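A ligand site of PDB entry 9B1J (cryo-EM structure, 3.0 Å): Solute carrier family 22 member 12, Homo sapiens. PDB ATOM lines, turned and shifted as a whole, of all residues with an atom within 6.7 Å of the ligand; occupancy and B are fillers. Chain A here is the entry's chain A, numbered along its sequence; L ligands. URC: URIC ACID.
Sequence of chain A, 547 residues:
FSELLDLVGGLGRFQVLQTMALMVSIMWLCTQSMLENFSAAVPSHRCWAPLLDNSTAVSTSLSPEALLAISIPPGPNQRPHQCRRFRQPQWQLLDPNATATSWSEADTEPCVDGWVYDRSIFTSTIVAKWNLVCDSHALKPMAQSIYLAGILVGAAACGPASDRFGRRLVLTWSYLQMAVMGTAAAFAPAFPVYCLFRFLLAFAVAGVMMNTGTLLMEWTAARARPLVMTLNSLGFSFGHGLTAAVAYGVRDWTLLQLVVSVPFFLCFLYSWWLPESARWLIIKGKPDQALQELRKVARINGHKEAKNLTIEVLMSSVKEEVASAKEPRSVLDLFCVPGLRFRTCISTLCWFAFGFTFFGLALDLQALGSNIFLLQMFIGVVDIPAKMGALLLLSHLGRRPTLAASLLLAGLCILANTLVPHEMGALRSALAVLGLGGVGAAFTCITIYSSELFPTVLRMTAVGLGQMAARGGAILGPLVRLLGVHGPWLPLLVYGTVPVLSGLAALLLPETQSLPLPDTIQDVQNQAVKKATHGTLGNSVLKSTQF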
ATOM      1  N   LEU A  29      -4.546  -6.348  30.186  1.00  0.00           N
ATOM      2  CA  LEU A  29      -5.743  -6.929  30.751  1.00  0.00           C
ATOM      3  C   LEU A  29      -6.651  -7.510  29.663  1.00  0.00           C
ATOM      4  O   LEU A  29      -7.319  -8.525  29.887  1.00  0.00           O
ATOM      5  CB  LEU A  29      -6.480  -5.862  31.569  1.00  0.00           C
ATOM      6  CG  LEU A  29      -7.864  -6.168  32.125  1.00  0.00           C
ATOM      7  CD1 LEU A  29      -7.997  -5.533  33.487  1.00  0.00           C
ATOM      8  CD2 LEU A  29      -8.933  -5.657  31.180  1.00  0.00           C
ATOM      9  N   CYS A  30      -6.698  -6.862  28.502  1.00  0.00           N
ATOM     10  CA  CYS A  30      -7.444  -7.425  27.372  1.00  0.00           C
ATOM     11  C   CYS A  30      -6.807  -8.716  26.873  1.00  0.00           C
ATOM     12  O   CYS A  30      -7.516  -9.650  26.475  1.00  0.00           O
ATOM     13  CB  CYS A  30      -7.528  -6.425  26.233  1.00  0.00           C
ATOM     14  SG  CYS A  30      -8.359  -7.097  24.783  1.00  0.00           S
ATOM     15  N   SER A  33      -8.018 -11.772  28.786  1.00  0.00           N
ATOM     16  CA  SER A  33      -9.315 -12.316  28.420  1.00  0.00           C
ATOM     17  C   SER A  33      -9.266 -13.026  27.069  1.00  0.00           C
ATOM     18  O   SER A  33      -9.799 -14.131  26.930  1.00  0.00           O
ATOM     19  CB  SER A  33     -10.372 -11.211  28.382  1.00  0.00           C
ATOM     20  OG  SER A  33     -10.394 -10.491  29.600  1.00  0.00           O
ATOM     21  N   MET A  34      -8.628 -12.417  26.077  1.00  0.00           N
ATOM     22  CA  MET A  34      -8.611 -13.016  24.738  1.00  0.00           C
ATOM     23  C   MET A  34      -7.666 -14.205  24.645  1.00  0.00           C
ATOM     24  O   MET A  34      -7.663 -14.895  23.622  1.00  0.00           O
ATOM     25  CB  MET A  34      -8.234 -11.977  23.685  1.00  0.00           C
ATOM     26  CG  MET A  34      -9.287 -10.902  23.486  1.00  0.00           C
ATOM     27  SD  MET A  34     -10.771 -11.522  22.662  1.00  0.00           S
ATOM     28  CE  MET A  34     -11.950 -11.430  23.996  1.00  0.00           C
ATOM     29  N   ILE A 151     -15.462 -12.907  36.738  1.00  0.00           N
ATOM     30  CA  ILE A 151     -15.566 -11.464  36.542  1.00  0.00           C
ATOM     31  C   ILE A 151     -16.885 -10.929  37.080  1.00  0.00           C
ATOM     32  O   ILE A 151     -16.946  -9.830  37.642  1.00  0.00           O
ATOM     33  CB  ILE A 151     -15.388 -11.073  35.064  1.00  0.00           C
ATOM     34  CG1 ILE A 151     -14.134 -11.708  34.469  1.00  0.00           C
ATOM     35  CG2 ILE A 151     -15.257  -9.559  34.971  1.00  0.00           C
ATOM     36  CD1 ILE A 151     -13.796 -11.226  33.079  1.00  0.00           C
ATOM     37  N   VAL A 205      -9.518  -8.993  37.595  1.00  0.00           N
ATOM     38  CA  VAL A 205      -9.755  -8.289  36.347  1.00  0.00           C
ATOM     39  C   VAL A 205     -10.924  -7.321  36.504  1.00  0.00           C
ATOM     40  O   VAL A 205     -10.885  -6.183  36.013  1.00  0.00           O
ATOM     41  CB  VAL A 205     -10.008  -9.287  35.205  1.00  0.00           C
ATOM     42  CG1 VAL A 205     -10.654  -8.588  34.017  1.00  0.00           C
ATOM     43  CG2 VAL A 205      -8.716  -9.959  34.787  1.00  0.00           C
ATOM     44  N   MET A 209     -10.794  -3.263  35.857  1.00  0.00           N
ATOM     45  CA  MET A 209     -11.669  -2.658  34.867  1.00  0.00           C
ATOM     46  C   MET A 209     -12.464  -1.510  35.468  1.00  0.00           C
ATOM     47  O   MET A 209     -12.519  -0.406  34.909  1.00  0.00           O
ATOM     48  CB  MET A 209     -12.634  -3.699  34.300  1.00  0.00           C
ATOM     49  CG  MET A 209     -12.038  -4.631  33.290  1.00  0.00           C
ATOM     50  SD  MET A 209     -13.267  -5.813  32.715  1.00  0.00           S
ATOM     51  CE  MET A 209     -12.334  -6.679  31.474  1.00  0.00           C
ATOM     52  N   SER A 233     -11.325   3.043  26.258  1.00  0.00           N
ATOM     53  CA  SER A 233     -11.958   1.985  25.471  1.00  0.00           C
ATOM     54  C   SER A 233     -11.107   1.546  24.284  1.00  0.00           C
ATOM     55  O   SER A 233     -11.239   0.390  23.855  1.00  0.00           O
ATOM     56  CB  SER A 233     -13.322   2.453  24.972  1.00  0.00           C
ATOM     57  OG  SER A 233     -14.179   2.780  26.062  1.00  0.00           O
ATOM     58  N   PHE A 236      -8.592  -1.578  24.838  1.00  0.00           N
ATOM     59  CA  PHE A 236      -8.945  -2.941  24.445  1.00  0.00           C
ATOM     60  C   PHE A 236      -8.676  -3.198  22.965  1.00  0.00           C
ATOM     61  O   PHE A 236      -8.254  -4.291  22.571  1.00  0.00           O
ATOM     62  CB  PHE A 236     -10.418  -3.215  24.756  1.00  0.00           C
ATOM     63  CG  PHE A 236     -10.738  -3.266  26.217  1.00  0.00           C
ATOM     64  CD1 PHE A 236     -10.533  -4.436  26.932  1.00  0.00           C
ATOM     65  CD2 PHE A 236     -11.259  -2.167  26.876  1.00  0.00           C
ATOM     66  CE1 PHE A 236     -10.832  -4.489  28.275  1.00  0.00           C
ATOM     67  CE2 PHE A 236     -11.552  -2.227  28.216  1.00  0.00           C
ATOM     68  CZ  PHE A 236     -11.341  -3.384  28.917  1.00  0.00           C
ATOM     69  N   SER A 237      -8.949  -2.190  22.124  1.00  0.00           N
ATOM     70  CA  SER A 237      -8.701  -2.343  20.696  1.00  0.00           C
ATOM     71  C   SER A 237      -7.246  -2.684  20.433  1.00  0.00           C
ATOM     72  O   SER A 237      -6.932  -3.578  19.641  1.00  0.00           O
ATOM     73  CB  SER A 237      -9.105  -1.071  19.970  1.00  0.00           C
ATOM     74  OG  SER A 237     -10.409  -0.668  20.334  1.00  0.00           O
ATOM     75  N   HIS A 240      -6.318  -6.340  21.460  1.00  0.00           N
ATOM     76  CA  HIS A 240      -6.508  -7.419  20.481  1.00  0.00           C
ATOM     77  C   HIS A 240      -5.258  -7.617  19.622  1.00  0.00           C
ATOM     78  O   HIS A 240      -4.777  -8.744  19.444  1.00  0.00           O
ATOM     79  CB  HIS A 240      -7.711  -7.127  19.597  1.00  0.00           C
ATOM     80  CG  HIS A 240      -9.020  -7.133  20.314  1.00  0.00           C
ATOM     81  ND1 HIS A 240      -9.589  -8.284  20.808  1.00  0.00           N
ATOM     82  CD2 HIS A 240      -9.882  -6.129  20.615  1.00  0.00           C
ATOM     83  CE1 HIS A 240     -10.745  -7.990  21.389  1.00  0.00           C
ATOM     84  NE2 HIS A 240     -10.937  -6.688  21.285  1.00  0.00           N
ATOM     85  N   PHE A 354     -24.395  -6.889  24.292  1.00  0.00           N
ATOM     86  CA  PHE A 354     -22.982  -6.712  23.997  1.00  0.00           C
ATOM     87  C   PHE A 354     -22.173  -7.884  24.508  1.00  0.00           C
ATOM     88  O   PHE A 354     -21.463  -8.545  23.747  1.00  0.00           O
ATOM     89  CB  PHE A 354     -22.426  -5.433  24.610  1.00  0.00           C
ATOM     90  CG  PHE A 354     -20.932  -5.448  24.707  1.00  0.00           C
ATOM     91  CD1 PHE A 354     -20.146  -5.159  23.601  1.00  0.00           C
ATOM     92  CD2 PHE A 354     -20.304  -5.796  25.896  1.00  0.00           C
ATOM     93  CE1 PHE A 354     -18.772  -5.199  23.683  1.00  0.00           C
ATOM     94  CE2 PHE A 354     -18.921  -5.825  25.977  1.00  0.00           C
ATOM     95  CZ  PHE A 354     -18.168  -5.524  24.867  1.00  0.00           C
ATOM     96  N   PHE A 358     -20.429 -10.588  22.047  1.00  0.00           N
ATOM     97  CA  PHE A 358     -18.986 -10.415  21.899  1.00  0.00           C
ATOM     98  C   PHE A 358     -18.228 -11.612  22.450  1.00  0.00           C
ATOM     99  O   PHE A 358     -17.306 -12.111  21.805  1.00  0.00           O
ATOM    100  CB  PHE A 358     -18.504  -9.135  22.577  1.00  0.00           C
ATOM    101  CG  PHE A 358     -17.117  -8.721  22.156  1.00  0.00           C
ATOM    102  CD1 PHE A 358     -16.929  -7.898  21.062  1.00  0.00           C
ATOM    103  CD2 PHE A 358     -16.002  -9.176  22.837  1.00  0.00           C
ATOM    104  CE1 PHE A 358     -15.660  -7.525  20.667  1.00  0.00           C
ATOM    105  CE2 PHE A 358     -14.733  -8.803  22.442  1.00  0.00           C
ATOM    106  CZ  PHE A 358     -14.565  -7.989  21.360  1.00  0.00           C
ATOM    107  N   PHE A 359     -18.568 -12.062  23.660  1.00  0.00           N
ATOM    108  CA  PHE A 359     -17.849 -13.204  24.200  1.00  0.00           C
ATOM    109  C   PHE A 359     -18.427 -14.533  23.756  1.00  0.00           C
ATOM    110  O   PHE A 359     -17.855 -15.585  24.092  1.00  0.00           O
ATOM    111  CB  PHE A 359     -17.790 -13.099  25.729  1.00  0.00           C
ATOM    112  CG  PHE A 359     -16.841 -12.022  26.210  1.00  0.00           C
ATOM    113  CD1 PHE A 359     -15.502 -12.318  26.431  1.00  0.00           C
ATOM    114  CD2 PHE A 359     -17.279 -10.728  26.409  1.00  0.00           C
ATOM    115  CE1 PHE A 359     -14.633 -11.328  26.860  1.00  0.00           C
ATOM    116  CE2 PHE A 359     -16.410  -9.748  26.829  1.00  0.00           C
ATOM    117  CZ  PHE A 359     -15.090 -10.054  27.062  1.00  0.00           C
ATOM    118  N   ALA A 362     -16.046 -13.775  19.887  1.00  0.00           N
ATOM    119  CA  ALA A 362     -14.634 -13.450  19.965  1.00  0.00           C
ATOM    120  C   ALA A 362     -13.786 -14.537  20.605  1.00  0.00           C
ATOM    121  O   ALA A 362     -12.560 -14.508  20.464  1.00  0.00           O
ATOM    122  CB  ALA A 362     -14.456 -12.152  20.752  1.00  0.00           C
ATOM    123  N   GLN A 376      -7.737 -12.268  14.835  1.00  0.00           N
ATOM    124  CA  GLN A 376      -7.678 -11.488  16.070  1.00  0.00           C
ATOM    125  C   GLN A 376      -7.081 -10.103  15.813  1.00  0.00           C
ATOM    126  O   GLN A 376      -7.620  -9.067  16.275  1.00  0.00           O
ATOM    127  CB  GLN A 376      -6.828 -12.273  17.076  1.00  0.00           C
ATOM    128  CG  GLN A 376      -6.593 -11.612  18.408  1.00  0.00           C
ATOM    129  CD  GLN A 376      -7.850 -11.546  19.247  1.00  0.00           C
ATOM    130  OE1 GLN A 376      -8.344 -10.472  19.554  1.00  0.00           O
ATOM    131  NE2 GLN A 376      -8.362 -12.705  19.620  1.00  0.00           N
ATOM    132  N   ILE A 379      -9.692  -8.086  14.323  1.00  0.00           N
ATOM    133  CA  ILE A 379     -10.707  -7.699  15.288  1.00  0.00           C
ATOM    134  C   ILE A 379     -10.258  -6.485  16.076  1.00  0.00           C
ATOM    135  O   ILE A 379     -11.081  -5.757  16.626  1.00  0.00           O
ATOM    136  CB  ILE A 379     -11.051  -8.883  16.204  1.00  0.00           C
ATOM    137  CG1 ILE A 379     -11.921  -9.886  15.462  1.00  0.00           C
ATOM    138  CG2 ILE A 379     -11.761  -8.405  17.456  1.00  0.00           C
ATOM    139  CD1 ILE A 379     -11.955 -11.262  16.069  1.00  0.00           C
ATOM    140  N   ASP A 383     -11.929  -2.688  14.957  1.00  0.00           N
ATOM    141  CA  ASP A 383     -12.586  -2.122  16.126  1.00  0.00           C
ATOM    142  C   ASP A 383     -12.261  -0.658  16.291  1.00  0.00           C
ATOM    143  O   ASP A 383     -13.107   0.113  16.758  1.00  0.00           O
ATOM    144  CB  ASP A 383     -12.194  -2.884  17.389  1.00  0.00           C
ATOM    145  CG  ASP A 383     -12.935  -2.379  18.608  1.00  0.00           C
ATOM    146  OD1 ASP A 383     -14.184  -2.355  18.578  1.00  0.00           O
ATOM    147  OD2 ASP A 383     -12.271  -2.016  19.603  1.00  0.00           O
ATOM    148  N   LYS A 387     -15.157   2.400  16.580  1.00  0.00           N
ATOM    149  CA  LYS A 387     -15.360   3.137  17.822  1.00  0.00           C
ATOM    150  C   LYS A 387     -15.282   4.640  17.601  1.00  0.00           C
ATOM    151  O   LYS A 387     -16.062   5.398  18.181  1.00  0.00           O
ATOM    152  CB  LYS A 387     -14.356   2.680  18.867  1.00  0.00           C
ATOM    153  CG  LYS A 387     -14.807   1.454  19.636  1.00  0.00           C
ATOM    154  CD  LYS A 387     -13.718   0.921  20.542  1.00  0.00           C
ATOM    155  CE  LYS A 387     -14.252  -0.227  21.383  1.00  0.00           C
ATOM    156  NZ  LYS A 387     -13.171  -1.061  21.977  1.00  0.00           N
ATOM    157  N   VAL A 439     -20.512  -4.639  17.403  1.00  0.00           N
ATOM    158  CA  VAL A 439     -20.698  -4.859  18.844  1.00  0.00           C
ATOM    159  C   VAL A 439     -19.767  -3.956  19.651  1.00  0.00           C
ATOM    160  O   VAL A 439     -20.173  -3.344  20.646  1.00  0.00           O
ATOM    161  CB  VAL A 439     -20.482  -6.344  19.187  1.00  0.00           C
ATOM    162  CG1 VAL A 439     -20.587  -6.566  20.687  1.00  0.00           C
ATOM    163  CG2 VAL A 439     -21.486  -7.210  18.437  1.00  0.00           C
ATOM    164  N   GLY A 440     -18.506  -3.862  19.236  1.00  0.00           N
ATOM    165  CA  GLY A 440     -17.563  -3.010  19.949  1.00  0.00           C
ATOM    166  C   GLY A 440     -17.925  -1.542  19.888  1.00  0.00           C
ATOM    167  O   GLY A 440     -17.671  -0.801  20.841  1.00  0.00           O
ATOM    168  N   ALA A 441     -18.523  -1.097  18.781  1.00  0.00           N
ATOM    169  CA  ALA A 441     -19.022   0.278  18.721  1.00  0.00           C
ATOM    170  C   ALA A 441     -20.197   0.482  19.671  1.00  0.00           C
ATOM    171  O   ALA A 441     -20.275   1.486  20.378  1.00  0.00           O
ATOM    172  CB  ALA A 441     -19.445   0.621  17.296  1.00  0.00           C
ATOM    173  N   PHE A 443     -20.589  -0.921  22.347  1.00  0.00           N
ATOM    174  CA  PHE A 443     -20.056  -0.846  23.703  1.00  0.00           C
ATOM    175  C   PHE A 443     -19.904   0.598  24.165  1.00  0.00           C
ATOM    176  O   PHE A 443     -20.451   1.005  25.204  1.00  0.00           O
ATOM    177  CB  PHE A 443     -18.717  -1.569  23.783  1.00  0.00           C
ATOM    178  CG  PHE A 443     -18.084  -1.541  25.141  1.00  0.00           C
ATOM    179  CD1 PHE A 443     -18.700  -2.163  26.215  1.00  0.00           C
ATOM    180  CD2 PHE A 443     -16.876  -0.899  25.347  1.00  0.00           C
ATOM    181  CE1 PHE A 443     -18.129  -2.136  27.464  1.00  0.00           C
ATOM    182  CE2 PHE A 443     -16.298  -0.868  26.603  1.00  0.00           C
ATOM    183  CZ  PHE A 443     -16.925  -1.491  27.657  1.00  0.00           C
ATOM    184  N   ARG A 471     -22.520  -8.871  32.187  1.00  0.00           N
ATOM    185  CA  ARG A 471     -21.734  -9.988  32.720  1.00  0.00           C
ATOM    186  C   ARG A 471     -22.542 -11.285  32.730  1.00  0.00           C
ATOM    187  O   ARG A 471     -22.018 -12.370  32.414  1.00  0.00           O
ATOM    188  CB  ARG A 471     -21.205  -9.614  34.095  1.00  0.00           C
ATOM    189  CG  ARG A 471     -20.064  -8.677  33.877  1.00  0.00           C
ATOM    190  CD  ARG A 471     -19.707  -7.742  34.995  1.00  0.00           C
ATOM    191  NE  ARG A 471     -18.499  -7.059  34.562  1.00  0.00           N
ATOM    192  CZ  ARG A 471     -18.153  -5.819  34.849  1.00  0.00           C
ATOM    193  NH1 ARG A 471     -18.883  -5.064  35.652  1.00  0.00           N
ATOM    194  NH2 ARG A 471     -17.050  -5.312  34.306  1.00  0.00           N
HETATM  195  N1  URC L   1     -13.131  -5.280  23.382  1.00  0.00           N
HETATM  196  C2  URC L   1     -14.063  -4.326  23.776  1.00  0.00           C
HETATM  197  C6  URC L   1     -12.814  -6.235  24.271  1.00  0.00           C
HETATM  198  N3  URC L   1     -14.778  -4.226  25.035  1.00  0.00           N
HETATM  199  O11 URC L   1     -14.371  -3.363  22.856  1.00  0.00           O
HETATM  200  C4  URC L   1     -14.425  -5.201  25.881  1.00  0.00           C
HETATM  201  C5  URC L   1     -13.433  -6.288  25.591  1.00  0.00           C
HETATM  202  N9  URC L   1     -14.907  -5.425  27.196  1.00  0.00           N
HETATM  203  O13 URC L   1     -11.916  -7.186  23.962  1.00  0.00           O
HETATM  204  N7  URC L   1     -13.306  -7.115  26.635  1.00  0.00           N
HETATM  205  C8  URC L   1     -14.208  -6.553  27.589  1.00  0.00           C
HETATM  206  O24 URC L   1     -14.355  -7.138  28.805  1.00  0.00           O
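NZ of Lys 387 sits at hydrogen-bond distance from O11 of the ligand, 2.7 Å away. An oxygen (O13) of the ligand is in hydrogen-bond range of the side-chain sulfur of Cys 30 (3.7 Å). NE2 of His 240 is in hydrogen-bond range of O13 of the ligand.
A ring nitrogen (ND1) of His 240 sits at hydrogen-bond distance from the side-chain amide oxygen (OE1) of Gln 376 (2.8 Å). The side-chain amino group (NZ) of Lys 387 is in hydrogen-bond range of the side-chain hydroxyl (OG) of Ser 237 (3.2 Å). NZ of Lys 387 lies within hydrogen-bond range of O of Ser 233 (3.1 Å). The side-chain sulfur (SG) of Cys 30 sits at hydrogen-bond distance from the backbone carbonyl oxygen (O) of Phe 236, 3.6 Å away. NZ of Lys 387 is in salt-bridge range of OD2 of Asp 383 (2.7 Å).
Met 209 touches the ligand. CB of Phe 236 touches N1 of the ligand, 3.7 Å away. Phe 354 touches the ligand (CZ to N3, 3.6 Å). Phe 358 touches the ligand. Phe 359 touches the ligand (CZ to N7, 3.5 Å). Phe 443 touches the ligand. Hydrophobic or aromatic side chains that line the ligand: Met 209, Phe 236, His 240, Phe 354, Phe 358, Phe 359 and Phe 443. Within 4 Å of the ligand: Cys 30, Met 209, Phe 236, His 240, Phe 354, Phe 358, Phe 359, Lys 387 and Phe 443. Along chain A the residues within 4 Å of the ligand span positions 30 to 443. The nearest printed residue that does not touch the ligand is Asp 383 (4.1 Å).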
